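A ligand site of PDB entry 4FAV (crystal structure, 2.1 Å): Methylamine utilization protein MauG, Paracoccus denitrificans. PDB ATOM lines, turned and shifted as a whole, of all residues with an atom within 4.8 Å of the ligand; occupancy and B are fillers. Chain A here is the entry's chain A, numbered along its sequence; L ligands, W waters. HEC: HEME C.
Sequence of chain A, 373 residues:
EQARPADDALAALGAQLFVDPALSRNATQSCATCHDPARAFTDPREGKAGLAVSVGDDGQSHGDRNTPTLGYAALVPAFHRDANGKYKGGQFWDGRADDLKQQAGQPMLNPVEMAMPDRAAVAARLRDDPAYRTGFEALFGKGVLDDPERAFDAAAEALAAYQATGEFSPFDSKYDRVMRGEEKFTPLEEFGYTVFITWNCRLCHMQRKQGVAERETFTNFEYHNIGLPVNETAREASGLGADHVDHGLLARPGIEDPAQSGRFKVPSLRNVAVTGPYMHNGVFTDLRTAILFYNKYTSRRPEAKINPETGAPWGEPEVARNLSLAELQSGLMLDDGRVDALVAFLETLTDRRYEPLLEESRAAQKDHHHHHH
N of Cys 31 lies within hydrogen-bond range of O of Phe 18, at 3.3 Å.
NH2 of Arg 45 sits at hydrogen-bond distance from SG of Cys 34, 3.4 Å away.
ND1 of His 35 sits at hydrogen-bond distance from O of Pro 68 (3.1 Å).
The backbone NH of Arg 96 lies within hydrogen-bond range of the backbone carbonyl oxygen of Gln 91 (3.4 Å).
O of Trp 93 sits at hydrogen-bond distance from N of Lys 265, at 3.0 Å.
The guanidinium group (NH1) of Arg 65 is in salt-bridge range of the side-chain carboxylate (OD1) of Asp 94.
The backbone carbonyl oxygen (O) of Glu 113 sits close to the side-chain amide nitrogen (NE2) of Gln 29 (3.5 Å).
OG of Ser 30 is in hydrogen-bond range of O of Phe 18.
The side-chain amide nitrogen (NE2) of Gln 103 sits close to a nitrogen (NA) of the ligand (3.2 Å).
Gln 29 touches the ligand.
Ser 30 touches the ligand.
Ser 54 touches the ligand.
Val 55 touches the ligand (O to CBC, 3.7 Å).
Thr 67 touches the ligand (OG1 to CHD, 3.2 Å).
Pro 68 touches the ligand.
CD2 of Leu 70 touches C4A of the ligand, 3.3 Å away.
Gln 91 touches the ligand.
Leu 100 touches the ligand (CD2 to CMA, 3.3 Å).
Ala 104 touches the ligand (O to CBB, 3.4 Å).
Pro 107 touches the ligand.
CE of Met 108 touches CBB of the ligand (3.95 Å).
CB of Glu 113 touches CBC of the ligand, 3.8 Å away.
Met 114 touches the ligand.
Gln 163 touches the ligand (NE2 to CMA, 3.1 Å).
Within 4 Å of the ligand: Gln 29, Ser 30, Cys 31, Cys 34, His 35, Ser 54, Val 55, Arg 65, Thr 67, Pro 68, Leu 70, Gln 91, Phe 92, Trp 93, Arg 96, Leu 100, Gln 103, Ala 104, Pro 107, Met 108, Glu 113, Met 114, Gln 163 and Lys 265.
Water W2 lies within hydrogen-bond range of an oxygen (O1A) of the ligand and the side-chain amino group of Lys 265.
The side-chain sulfur of Cys 31 is covalently linked to a carbon (CAB) of the ligand (1.8 Å).
SG of Cys 34 is covalently linked to CAC of the ligand (1.8 Å).
NE2 of His 35 is bound to FE of the ligand, 2.0 Å away.
O1D of the ligand is in salt-bridge range of NH2 of Arg 96 (2.4 Å).
An oxygen (O2A) of the ligand sits at hydrogen-bond distance from the backbone NH (N) of Phe 92 (2.9 Å).
An oxygen (O2A) of the ligand is in salt-bridge range of the side-chain amino group of Lys 265 (3.1 Å).
The backbone NH of Trp 93 sits at hydrogen-bond distance from an oxygen (O2D) of the ligand (3.1 Å).
NH1 of Arg 65 is in salt-bridge range of O1D of the ligand, at 3.1 Å.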
ATOM      1  N   PHE A  18     -12.252  21.399 -13.066  1.00  0.00           N
ATOM      2  CA  PHE A  18     -11.270  22.074 -12.242  1.00  0.00           C
ATOM      3  C   PHE A  18     -10.130  22.596 -13.122  1.00  0.00           C
ATOM      4  O   PHE A  18      -9.467  23.611 -12.795  1.00  0.00           O
ATOM      5  CB  PHE A  18     -10.709  21.075 -11.261  1.00  0.00           C
ATOM      6  CG  PHE A  18      -9.765  21.661 -10.299  1.00  0.00           C
ATOM      7  CD1 PHE A  18     -10.230  22.157  -9.084  1.00  0.00           C
ATOM      8  CD2 PHE A  18      -8.393  21.699 -10.561  1.00  0.00           C
ATOM      9  CE1 PHE A  18      -9.370  22.689  -8.152  1.00  0.00           C
ATOM     10  CE2 PHE A  18      -7.514  22.267  -9.622  1.00  0.00           C
ATOM     11  CZ  PHE A  18      -8.015  22.740  -8.436  1.00  0.00           C
ATOM     12  N   GLN A  29      -8.780  31.204 -17.786  1.00  0.00           N
ATOM     13  CA  GLN A  29      -8.494  30.881 -16.366  1.00  0.00           C
ATOM     14  C   GLN A  29      -9.403  29.764 -15.810  1.00  0.00           C
ATOM     15  O   GLN A  29     -10.617  29.772 -16.059  1.00  0.00           O
ATOM     16  CB  GLN A  29      -8.694  32.123 -15.513  1.00  0.00           C
ATOM     17  CG  GLN A  29      -8.446  31.948 -14.008  1.00  0.00           C
ATOM     18  CD  GLN A  29      -8.324  33.269 -13.287  1.00  0.00           C
ATOM     19  OE1 GLN A  29      -7.275  33.923 -13.337  1.00  0.00           O
ATOM     20  NE2 GLN A  29      -9.389  33.669 -12.573  1.00  0.00           N
ATOM     21  N   SER A  30      -8.828  28.815 -15.079  1.00  0.00           N
ATOM     22  CA  SER A  30      -9.631  27.767 -14.437  1.00  0.00           C
ATOM     23  C   SER A  30      -9.287  27.746 -12.973  1.00  0.00           C
ATOM     24  O   SER A  30      -8.407  28.506 -12.561  1.00  0.00           O
ATOM     25  CB  SER A  30      -9.313  26.430 -15.069  1.00  0.00           C
ATOM     26  OG  SER A  30      -8.052  26.018 -14.617  1.00  0.00           O
ATOM     27  N   CYS A  31      -9.919  26.855 -12.188  1.00  0.00           N
ATOM     28  CA  CYS A  31      -9.541  26.750 -10.751  1.00  0.00           C
ATOM     29  C   CYS A  31      -8.053  26.473 -10.616  1.00  0.00           C
ATOM     30  O   CYS A  31      -7.353  27.038  -9.733  1.00  0.00           O
ATOM     31  CB  CYS A  31     -10.241  25.580 -10.088  1.00  0.00           C
ATOM     32  SG  CYS A  31     -12.014  25.451 -10.318  1.00  0.00           S
ATOM     33  N   CYS A  34      -5.140  29.094 -10.385  1.00  0.00           N
ATOM     34  CA  CYS A  34      -4.797  29.778  -9.162  1.00  0.00           C
ATOM     35  C   CYS A  34      -4.401  28.723  -8.163  1.00  0.00           C
ATOM     36  O   CYS A  34      -3.507  28.924  -7.341  1.00  0.00           O
ATOM     37  CB  CYS A  34      -5.976  30.573  -8.634  1.00  0.00           C
ATOM     38  SG  CYS A  34      -6.279  32.118  -9.477  1.00  0.00           S
ATOM     39  N   HIS A  35      -5.098  27.597  -8.220  1.00  0.00           N
ATOM     40  CA  HIS A  35      -4.763  26.522  -7.351  1.00  0.00           C
ATOM     41  C   HIS A  35      -3.992  25.528  -8.203  1.00  0.00           C
ATOM     42  O   HIS A  35      -4.493  24.448  -8.579  1.00  0.00           O
ATOM     43  CB  HIS A  35      -6.006  25.926  -6.714  1.00  0.00           C
ATOM     44  CG  HIS A  35      -6.831  26.907  -5.921  1.00  0.00           C
ATOM     45  ND1 HIS A  35      -6.597  27.169  -4.593  1.00  0.00           N
ATOM     46  CD2 HIS A  35      -7.907  27.649  -6.257  1.00  0.00           C
ATOM     47  CE1 HIS A  35      -7.515  27.998  -4.120  1.00  0.00           C
ATOM     48  NE2 HIS A  35      -8.342  28.294  -5.099  1.00  0.00           N
ATOM     49  N   ARG A  45       1.848  32.264 -10.014  1.00  0.00           N
ATOM     50  CA  ARG A  45       1.932  33.418 -10.952  1.00  0.00           C
ATOM     51  C   ARG A  45       2.298  34.737 -10.251  1.00  0.00           C
ATOM     52  O   ARG A  45       1.653  35.116  -9.273  1.00  0.00           O
ATOM     53  CB  ARG A  45       0.623  33.596 -11.754  1.00  0.00           C
ATOM     54  CG  ARG A  45       0.316  32.543 -12.845  1.00  0.00           C
ATOM     55  CD  ARG A  45      -1.133  32.693 -13.388  1.00  0.00           C
ATOM     56  NE  ARG A  45      -2.101  32.966 -12.301  1.00  0.00           N
ATOM     57  CZ  ARG A  45      -3.226  33.684 -12.431  1.00  0.00           C
ATOM     58  NH1 ARG A  45      -3.568  34.211 -13.639  1.00  0.00           N
ATOM     59  NH2 ARG A  45      -4.005  33.892 -11.368  1.00  0.00           N
ATOM     60  N   SER A  54      -3.678  36.797  -6.050  1.00  0.00           N
ATOM     61  CA  SER A  54      -3.871  36.307  -7.410  1.00  0.00           C
ATOM     62  C   SER A  54      -4.644  37.255  -8.311  1.00  0.00           C
ATOM     63  O   SER A  54      -5.503  38.032  -7.794  1.00  0.00           O
ATOM     64  CB  SER A  54      -4.536  34.948  -7.371  1.00  0.00           C
ATOM     65  OG  SER A  54      -3.679  34.037  -6.742  1.00  0.00           O
ATOM     66  N   VAL A  55      -4.356  37.174  -9.619  1.00  0.00           N
ATOM     67  CA  VAL A  55      -5.038  37.952 -10.652  1.00  0.00           C
ATOM     68  C   VAL A  55      -6.230  37.239 -11.295  1.00  0.00           C
ATOM     69  O   VAL A  55      -6.125  36.087 -11.772  1.00  0.00           O
ATOM     70  CB  VAL A  55      -4.042  38.274 -11.797  1.00  0.00           C
ATOM     71  CG1 VAL A  55      -4.699  39.158 -12.885  1.00  0.00           C
ATOM     72  CG2 VAL A  55      -2.815  38.941 -11.245  1.00  0.00           C
ATOM     73  N   GLY A  56      -7.373  37.920 -11.390  1.00  0.00           N
ATOM     74  CA  GLY A  56      -8.506  37.373 -12.131  1.00  0.00           C
ATOM     75  C   GLY A  56      -8.344  37.139 -13.647  1.00  0.00           C
ATOM     76  O   GLY A  56      -7.345  37.526 -14.282  1.00  0.00           O
ATOM     77  N   ARG A  65      -6.660  38.744  -0.623  1.00  0.00           N
ATOM     78  CA  ARG A  65      -6.159  37.609   0.174  1.00  0.00           C
ATOM     79  C   ARG A  65      -5.285  36.671  -0.651  1.00  0.00           C
ATOM     80  O   ARG A  65      -5.447  36.575  -1.859  1.00  0.00           O
ATOM     81  CB  ARG A  65      -7.320  36.827   0.801  1.00  0.00           C
ATOM     82  CG  ARG A  65      -8.226  37.735   1.652  1.00  0.00           C
ATOM     83  CD  ARG A  65      -8.729  36.985   2.816  1.00  0.00           C
ATOM     84  NE  ARG A  65      -9.614  37.839   3.603  1.00  0.00           N
ATOM     85  CZ  ARG A  65     -10.891  37.573   3.842  1.00  0.00           C
ATOM     86  NH1 ARG A  65     -11.448  36.444   3.385  1.00  0.00           N
ATOM     87  NH2 ARG A  65     -11.611  38.402   4.569  1.00  0.00           N
ATOM     88  N   ASN A  66      -4.385  35.968   0.040  1.00  0.00           N
ATOM     89  CA  ASN A  66      -3.497  34.996  -0.578  1.00  0.00           C
ATOM     90  C   ASN A  66      -4.249  33.706  -0.813  1.00  0.00           C
ATOM     91  O   ASN A  66      -5.124  33.315   0.028  1.00  0.00           O
ATOM     92  CB  ASN A  66      -2.291  34.749   0.317  1.00  0.00           C
ATOM     93  CG  ASN A  66      -1.421  33.643  -0.188  1.00  0.00           C
ATOM     94  OD1 ASN A  66      -1.322  32.577   0.444  1.00  0.00           O
ATOM     95  ND2 ASN A  66      -0.831  33.848  -1.394  1.00  0.00           N
ATOM     96  N   THR A  67      -3.936  33.073  -1.959  1.00  0.00           N
ATOM     97  CA  THR A  67      -4.608  31.872  -2.457  1.00  0.00           C
ATOM     98  C   THR A  67      -4.158  30.691  -1.594  1.00  0.00           C
ATOM     99  O   THR A  67      -2.976  30.372  -1.541  1.00  0.00           O
ATOM    100  CB  THR A  67      -4.314  31.685  -3.960  1.00  0.00           C
ATOM    101  OG1 THR A  67      -4.932  32.744  -4.723  1.00  0.00           O
ATOM    102  CG2 THR A  67      -4.756  30.273  -4.514  1.00  0.00           C
ATOM    103  N   PRO A  68      -5.090  30.119  -0.777  1.00  0.00           N
ATOM    104  CA  PRO A  68      -4.686  28.985   0.009  1.00  0.00           C
ATOM    105  C   PRO A  68      -4.648  27.667  -0.779  1.00  0.00           C
ATOM    106  O   PRO A  68      -5.288  27.493  -1.821  1.00  0.00           O
ATOM    107  CB  PRO A  68      -5.781  28.933   1.135  1.00  0.00           C
ATOM    108  CG  PRO A  68      -7.007  29.422   0.402  1.00  0.00           C
ATOM    109  CD  PRO A  68      -6.528  30.352  -0.731  1.00  0.00           C
ATOM    110  N   THR A  69      -3.876  26.713  -0.268  1.00  0.00           N
ATOM    111  CA  THR A  69      -3.894  25.350  -0.799  1.00  0.00           C
ATOM    112  C   THR A  69      -5.287  24.694  -0.674  1.00  0.00           C
ATOM    113  O   THR A  69      -6.055  25.028   0.205  1.00  0.00           O
ATOM    114  CB  THR A  69      -2.987  24.491  -0.026  1.00  0.00           C
ATOM    115  OG1 THR A  69      -2.991  23.231  -0.662  1.00  0.00           O
ATOM    116  CG2 THR A  69      -3.575  24.352   1.512  1.00  0.00           C
ATOM    117  N   LEU A  70      -5.614  23.777  -1.565  1.00  0.00           N
ATOM    118  CA  LEU A  70      -6.865  23.027  -1.456  1.00  0.00           C
ATOM    119  C   LEU A  70      -6.585  21.648  -0.832  1.00  0.00           C
ATOM    120  O   LEU A  70      -7.525  20.910  -0.550  1.00  0.00           O
ATOM    121  CB  LEU A  70      -7.574  22.862  -2.813  1.00  0.00           C
ATOM    122  CG  LEU A  70      -7.882  24.161  -3.590  1.00  0.00           C
ATOM    123  CD1 LEU A  70      -8.684  23.905  -4.861  1.00  0.00           C
ATOM    124  CD2 LEU A  70      -8.598  25.159  -2.762  1.00  0.00           C
ATOM    125  N   ALA A  73      -8.266  20.518   2.556  1.00  0.00           N
ATOM    126  CA  ALA A  73      -9.394  21.413   2.793  1.00  0.00           C
ATOM    127  C   ALA A  73     -10.649  20.585   3.061  1.00  0.00           C
ATOM    128  O   ALA A  73     -11.538  21.008   3.784  1.00  0.00           O
ATOM    129  CB  ALA A  73      -9.609  22.418   1.663  1.00  0.00           C
ATOM    130  N   GLN A  91     -14.913  27.572   4.980  1.00  0.00           N
ATOM    131  CA  GLN A  91     -13.904  27.720   3.931  1.00  0.00           C
ATOM    132  C   GLN A  91     -13.736  29.198   3.618  1.00  0.00           C
ATOM    133  O   GLN A  91     -14.638  29.994   3.885  1.00  0.00           O
ATOM    134  CB  GLN A  91     -14.330  26.986   2.643  1.00  0.00           C
ATOM    135  CG  GLN A  91     -14.485  25.472   2.742  1.00  0.00           C
ATOM    136  CD  GLN A  91     -13.200  24.691   3.065  1.00  0.00           C
ATOM    137  OE1 GLN A  91     -13.265  23.618   3.660  1.00  0.00           O
ATOM    138  NE2 GLN A  91     -12.075  25.217   2.715  1.00  0.00           N
ATOM    139  N   PHE A  92     -12.602  29.506   2.986  1.00  0.00           N
ATOM    140  CA  PHE A  92     -12.010  30.861   2.900  1.00  0.00           C
ATOM    141  C   PHE A  92     -11.387  31.195   4.241  1.00  0.00           C
ATOM    142  O   PHE A  92     -11.833  30.690   5.296  1.00  0.00           O
ATOM    143  CB  PHE A  92     -13.001  31.989   2.590  1.00  0.00           C
ATOM    144  CG  PHE A  92     -13.643  31.890   1.243  1.00  0.00           C
ATOM    145  CD1 PHE A  92     -12.884  31.930   0.097  1.00  0.00           C
ATOM    146  CD2 PHE A  92     -15.023  31.766   1.139  1.00  0.00           C
ATOM    147  CE1 PHE A  92     -13.467  31.849  -1.172  1.00  0.00           C
ATOM    148  CE2 PHE A  92     -15.618  31.694  -0.130  1.00  0.00           C
ATOM    149  CZ  PHE A  92     -14.834  31.720  -1.267  1.00  0.00           C
ATOM    150  N   TRP A  93     -10.467  32.149   4.191  1.00  0.00           N
ATOM    151  CA  TRP A  93      -9.743  32.563   5.353  1.00  0.00           C
ATOM    152  C   TRP A  93     -10.659  33.192   6.407  1.00  0.00           C
ATOM    153  O   TRP A  93     -10.285  33.277   7.583  1.00  0.00           O
ATOM    154  CB  TRP A  93      -8.766  33.603   4.908  1.00  0.00           C
ATOM    155  CG  TRP A  93      -7.547  33.138   4.199  1.00  0.00           C
ATOM    156  CD1 TRP A  93      -7.282  33.229   2.839  1.00  0.00           C
ATOM    157  CD2 TRP A  93      -6.389  32.619   4.808  1.00  0.00           C
ATOM    158  NE1 TRP A  93      -6.014  32.759   2.576  1.00  0.00           N
ATOM    159  CE2 TRP A  93      -5.437  32.394   3.765  1.00  0.00           C
ATOM    160  CE3 TRP A  93      -6.028  32.341   6.136  1.00  0.00           C
ATOM    161  CZ2 TRP A  93      -4.147  31.872   4.029  1.00  0.00           C
ATOM    162  CZ3 TRP A  93      -4.730  31.817   6.388  1.00  0.00           C
ATOM    163  CH2 TRP A  93      -3.813  31.627   5.343  1.00  0.00           C
ATOM    164  N   ASP A  94     -11.840  33.640   6.002  1.00  0.00           N
ATOM    165  CA  ASP A  94     -12.779  34.288   6.929  1.00  0.00           C
ATOM    166  C   ASP A  94     -13.985  33.453   7.178  1.00  0.00           C
ATOM    167  O   ASP A  94     -14.984  33.936   7.697  1.00  0.00           O
ATOM    168  CB  ASP A  94     -13.187  35.682   6.466  1.00  0.00           C
ATOM    169  CG  ASP A  94     -13.811  35.703   5.083  1.00  0.00           C
ATOM    170  OD1 ASP A  94     -14.003  36.808   4.555  1.00  0.00           O
ATOM    171  OD2 ASP A  94     -14.126  34.652   4.511  1.00  0.00           O
ATOM    172  N   ARG A  96     -16.313  32.482   5.463  1.00  0.00           N
ATOM    173  CA  ARG A  96     -17.579  32.936   4.927  1.00  0.00           C
ATOM    174  C   ARG A  96     -18.338  31.875   4.062  1.00  0.00           C
ATOM    175  O   ARG A  96     -19.530  32.007   3.881  1.00  0.00           O
ATOM    176  CB  ARG A  96     -17.427  34.249   4.175  1.00  0.00           C
ATOM    177  CG  ARG A  96     -16.736  34.106   2.828  1.00  0.00           C
ATOM    178  CD  ARG A  96     -16.582  35.492   2.120  1.00  0.00           C
ATOM    179  NE  ARG A  96     -16.040  35.385   0.774  1.00  0.00           N
ATOM    180  CZ  ARG A  96     -14.742  35.288   0.521  1.00  0.00           C
ATOM    181  NH1 ARG A  96     -14.301  35.175  -0.727  1.00  0.00           N
ATOM    182  NH2 ARG A  96     -13.888  35.299   1.550  1.00  0.00           N
ATOM    183  N   LEU A 100     -16.992  23.069   1.235  1.00  0.00           N
ATOM    184  CA  LEU A 100     -16.396  23.167  -0.124  1.00  0.00           C
ATOM    185  C   LEU A 100     -17.444  23.404  -1.188  1.00  0.00           C
ATOM    186  O   LEU A 100     -17.209  24.134  -2.141  1.00  0.00           O
ATOM    187  CB  LEU A 100     -15.650  21.903  -0.497  1.00  0.00           C
ATOM    188  CG  LEU A 100     -14.413  21.687   0.331  1.00  0.00           C
ATOM    189  CD1 LEU A 100     -13.975  20.218   0.121  1.00  0.00           C
ATOM    190  CD2 LEU A 100     -13.374  22.739  -0.067  1.00  0.00           C
ATOM    191  N   GLN A 103     -18.449  26.856  -1.289  1.00  0.00           N
ATOM    192  CA  GLN A 103     -17.327  27.652  -1.731  1.00  0.00           C
ATOM    193  C   GLN A 103     -17.149  27.619  -3.293  1.00  0.00           C
ATOM    194  O   GLN A 103     -16.937  28.665  -3.892  1.00  0.00           O
ATOM    195  CB  GLN A 103     -16.059  27.256  -0.989  1.00  0.00           C
ATOM    196  CG  GLN A 103     -14.911  28.225  -1.240  1.00  0.00           C
ATOM    197  CD  GLN A 103     -14.359  28.062  -2.657  1.00  0.00           C
ATOM    198  OE1 GLN A 103     -14.484  26.995  -3.266  1.00  0.00           O
ATOM    199  NE2 GLN A 103     -13.737  29.089  -3.159  1.00  0.00           N
ATOM    200  N   ALA A 104     -17.290  26.448  -3.934  1.00  0.00           N
ATOM    201  CA  ALA A 104     -16.854  26.200  -5.314  1.00  0.00           C
ATOM    202  C   ALA A 104     -17.358  27.204  -6.319  1.00  0.00           C
ATOM    203  O   ALA A 104     -16.624  27.654  -7.198  1.00  0.00           O
ATOM    204  CB  ALA A 104     -17.195  24.744  -5.773  1.00  0.00           C
ATOM    205  N   PRO A 107     -15.740  31.514  -6.757  1.00  0.00           N
ATOM    206  CA  PRO A 107     -14.742  31.978  -7.782  1.00  0.00           C
ATOM    207  C   PRO A 107     -15.289  32.129  -9.205  1.00  0.00           C
ATOM    208  O   PRO A 107     -14.929  33.067  -9.892  1.00  0.00           O
ATOM    209  CB  PRO A 107     -13.665  30.865  -7.748  1.00  0.00           C
ATOM    210  CG  PRO A 107     -13.914  30.111  -6.437  1.00  0.00           C
ATOM    211  CD  PRO A 107     -15.358  30.213  -6.186  1.00  0.00           C
ATOM    212  N   MET A 108     -16.127  31.200  -9.655  1.00  0.00           N
ATOM    213  CA  MET A 108     -16.755  31.298 -10.973  1.00  0.00           C
ATOM    214  C   MET A 108     -17.392  32.651 -11.207  1.00  0.00           C
ATOM    215  O   MET A 108     -17.286  33.222 -12.302  1.00  0.00           O
ATOM    216  CB  MET A 108     -17.808  30.218 -11.189  1.00  0.00           C
ATOM    217  CG  MET A 108     -17.185  28.871 -11.513  1.00  0.00           C
ATOM    218  SD  MET A 108     -18.353  27.502 -11.627  1.00  0.00           S
ATOM    219  CE  MET A 108     -17.959  26.600 -10.140  1.00  0.00           C
ATOM    220  N   VAL A 112     -13.443  39.697  -9.683  1.00  0.00           N
ATOM    221  CA  VAL A 112     -11.974  39.808  -9.520  1.00  0.00           C
ATOM    222  C   VAL A 112     -11.235  38.447  -9.718  1.00  0.00           C
ATOM    223  O   VAL A 112      -9.997  38.382  -9.649  1.00  0.00           O
ATOM    224  CB  VAL A 112     -11.509  40.557  -8.150  1.00  0.00           C
ATOM    225  CG1 VAL A 112     -12.590  41.533  -7.596  1.00  0.00           C
ATOM    226  CG2 VAL A 112     -11.068  39.584  -7.055  1.00  0.00           C
ATOM    227  N   GLU A 113     -12.007  37.379  -9.923  1.00  0.00           N
ATOM    228  CA  GLU A 113     -11.485  36.048 -10.230  1.00  0.00           C
ATOM    229  C   GLU A 113     -11.964  35.625 -11.621  1.00  0.00           C
ATOM    230  O   GLU A 113     -11.687  36.305 -12.644  1.00  0.00           O
ATOM    231  CB  GLU A 113     -11.820  35.027  -9.105  1.00  0.00           C
ATOM    232  CG  GLU A 113     -11.470  35.621  -7.689  1.00  0.00           C
ATOM    233  CD  GLU A 113     -11.633  34.638  -6.484  1.00  0.00           C
ATOM    234  OE1 GLU A 113     -12.438  33.675  -6.519  1.00  0.00           O
ATOM    235  OE2 GLU A 113     -10.894  34.840  -5.491  1.00  0.00           O
ATOM    236  N   MET A 114     -12.712  34.549 -11.692  1.00  0.00           N
ATOM    237  CA  MET A 114     -13.094  33.969 -12.978  1.00  0.00           C
ATOM    238  C   MET A 114     -14.119  34.812 -13.732  1.00  0.00           C
ATOM    239  O   MET A 114     -14.149  34.776 -14.963  1.00  0.00           O
ATOM    240  CB  MET A 114     -13.559  32.522 -12.799  1.00  0.00           C
ATOM    241  CG  MET A 114     -12.473  31.714 -12.077  1.00  0.00           C
ATOM    242  SD  MET A 114     -12.921  30.036 -11.693  1.00  0.00           S
ATOM    243  CE  MET A 114     -12.979  29.378 -13.344  1.00  0.00           C
ATOM    244  N   LEU A 159     -16.916  19.755  -8.193  1.00  0.00           N
ATOM    245  CA  LEU A 159     -15.684  20.322  -7.625  1.00  0.00           C
ATOM    246  C   LEU A 159     -15.373  19.877  -6.168  1.00  0.00           C
ATOM    247  O   LEU A 159     -14.218  19.480  -5.845  1.00  0.00           O
ATOM    248  CB  LEU A 159     -15.735  21.820  -7.728  1.00  0.00           C
ATOM    249  CG  LEU A 159     -15.439  22.110  -9.242  1.00  0.00           C
ATOM    250  CD1 LEU A 159     -15.970  23.489  -9.538  1.00  0.00           C
ATOM    251  CD2 LEU A 159     -13.903  21.971  -9.726  1.00  0.00           C
ATOM    252  N   GLN A 163     -12.411  17.715  -4.769  1.00  0.00           N
ATOM    253  CA  GLN A 163     -11.420  18.111  -3.714  1.00  0.00           C
ATOM    254  C   GLN A 163     -11.392  17.160  -2.473  1.00  0.00           C
ATOM    255  O   GLN A 163     -10.537  17.318  -1.578  1.00  0.00           O
ATOM    256  CB  GLN A 163     -11.560  19.571  -3.227  1.00  0.00           C
ATOM    257  CG  GLN A 163     -11.392  20.640  -4.287  1.00  0.00           C
ATOM    258  CD  GLN A 163     -12.136  21.907  -3.947  1.00  0.00           C
ATOM    259  OE1 GLN A 163     -13.315  22.023  -4.254  1.00  0.00           O
ATOM    260  NE2 GLN A 163     -11.475  22.865  -3.319  1.00  0.00           N
ATOM    261  N   LYS A 265      -9.171  31.960   9.977  1.00  0.00           N
ATOM    262  CA  LYS A 265      -9.123  30.514  10.215  1.00  0.00           C
ATOM    263  C   LYS A 265      -7.690  30.044  10.370  1.00  0.00           C
ATOM    264  O   LYS A 265      -6.856  30.390   9.592  1.00  0.00           O
ATOM    265  CB  LYS A 265      -9.780  29.775   9.041  1.00  0.00           C
ATOM    266  CG  LYS A 265      -9.788  28.223   9.086  1.00  0.00           C
ATOM    267  CD  LYS A 265     -10.877  27.691   8.108  1.00  0.00           C
ATOM    268  CE  LYS A 265     -10.562  27.959   6.617  1.00  0.00           C
ATOM    269  NZ  LYS A 265      -9.158  27.620   6.046  1.00  0.00           N
HETATM  270 FE   HEC L   1     -10.016  29.382  -4.956  1.00  0.00          FE
HETATM  271  CHA HEC L   1     -10.017  30.029  -1.619  1.00  0.00           C
HETATM  272  CHB HEC L   1     -11.474  26.364  -4.409  1.00  0.00           C
HETATM  273  CHC HEC L   1     -10.817  29.258  -8.302  1.00  0.00           C
HETATM  274  CHD HEC L   1      -7.922  31.987  -5.486  1.00  0.00           C
HETATM  275  NA  HEC L   1     -10.652  28.334  -3.261  1.00  0.00           N
HETATM  276  C1A HEC L   1     -10.548  28.717  -1.980  1.00  0.00           C
HETATM  277  C2A HEC L   1     -11.027  27.707  -1.016  1.00  0.00           C
HETATM  278  C3A HEC L   1     -11.466  26.673  -1.830  1.00  0.00           C
HETATM  279  C4A HEC L   1     -11.177  27.128  -3.208  1.00  0.00           C
HETATM  280  CMA HEC L   1     -12.025  25.343  -1.472  1.00  0.00           C
HETATM  281  CAA HEC L   1     -11.002  27.802   0.475  1.00  0.00           C
HETATM  282  CBA HEC L   1      -9.763  27.040   0.962  1.00  0.00           C
HETATM  283  CGA HEC L   1      -9.434  27.295   2.461  1.00  0.00           C
HETATM  284  O1A HEC L   1      -8.444  26.731   2.959  1.00  0.00           O
HETATM  285  O2A HEC L   1     -10.093  28.087   3.163  1.00  0.00           O
HETATM  286  NB  HEC L   1     -10.995  28.020  -6.148  1.00  0.00           N
HETATM  287  C1B HEC L   1     -11.557  26.888  -5.789  1.00  0.00           C
HETATM  288  C2B HEC L   1     -12.283  26.222  -6.914  1.00  0.00           C
HETATM  289  C3B HEC L   1     -12.103  27.045  -8.007  1.00  0.00           C
HETATM  290  C4B HEC L   1     -11.286  28.146  -7.471  1.00  0.00           C
HETATM  291  CMB HEC L   1     -13.072  24.922  -6.885  1.00  0.00           C
HETATM  292  CAB HEC L   1     -12.639  26.842  -9.392  1.00  0.00           C
HETATM  293  CBB HEC L   1     -14.116  27.143  -9.387  1.00  0.00           C
HETATM  294  NC  HEC L   1      -9.446  30.447  -6.619  1.00  0.00           N
HETATM  295  C1C HEC L   1      -9.834  30.274  -7.896  1.00  0.00           C
HETATM  296  C2C HEC L   1      -9.166  31.207  -8.847  1.00  0.00           C
HETATM  297  C3C HEC L   1      -8.340  32.003  -8.053  1.00  0.00           C
HETATM  298  C4C HEC L   1      -8.596  31.498  -6.690  1.00  0.00           C
HETATM  299  CMC HEC L   1      -9.375  31.232 -10.352  1.00  0.00           C
HETATM  300  CAC HEC L   1      -7.403  33.132  -8.491  1.00  0.00           C
HETATM  301  CBC HEC L   1      -8.127  34.203  -9.255  1.00  0.00           C
HETATM  302  ND  HEC L   1      -9.023  30.751  -3.747  1.00  0.00           N
HETATM  303  C1D HEC L   1      -8.417  31.847  -4.116  1.00  0.00           C
HETATM  304  C2D HEC L   1      -8.243  32.875  -3.074  1.00  0.00           C
HETATM  305  C3D HEC L   1      -8.882  32.335  -1.979  1.00  0.00           C
HETATM  306  C4D HEC L   1      -9.333  31.015  -2.482  1.00  0.00           C
HETATM  307  CMD HEC L   1      -7.573  34.219  -3.227  1.00  0.00           C
HETATM  308  CAD HEC L   1      -9.068  32.882  -0.574  1.00  0.00           C
HETATM  309  CBD HEC L   1      -9.906  34.163  -0.651  1.00  0.00           C
HETATM  310  CGD HEC L   1     -10.653  34.468   0.633  1.00  0.00           C
HETATM  311  O1D HEC L   1     -11.666  35.218   0.556  1.00  0.00           O
HETATM  312  O2D HEC L   1     -10.265  33.971   1.708  1.00  0.00           O
HETATM  313  O   HOH W   1     -11.764  32.301  -4.216  1.00  0.00           O
HETATM  314  O   HOH W   2      -6.035  26.365   5.182  1.00  0.00           O
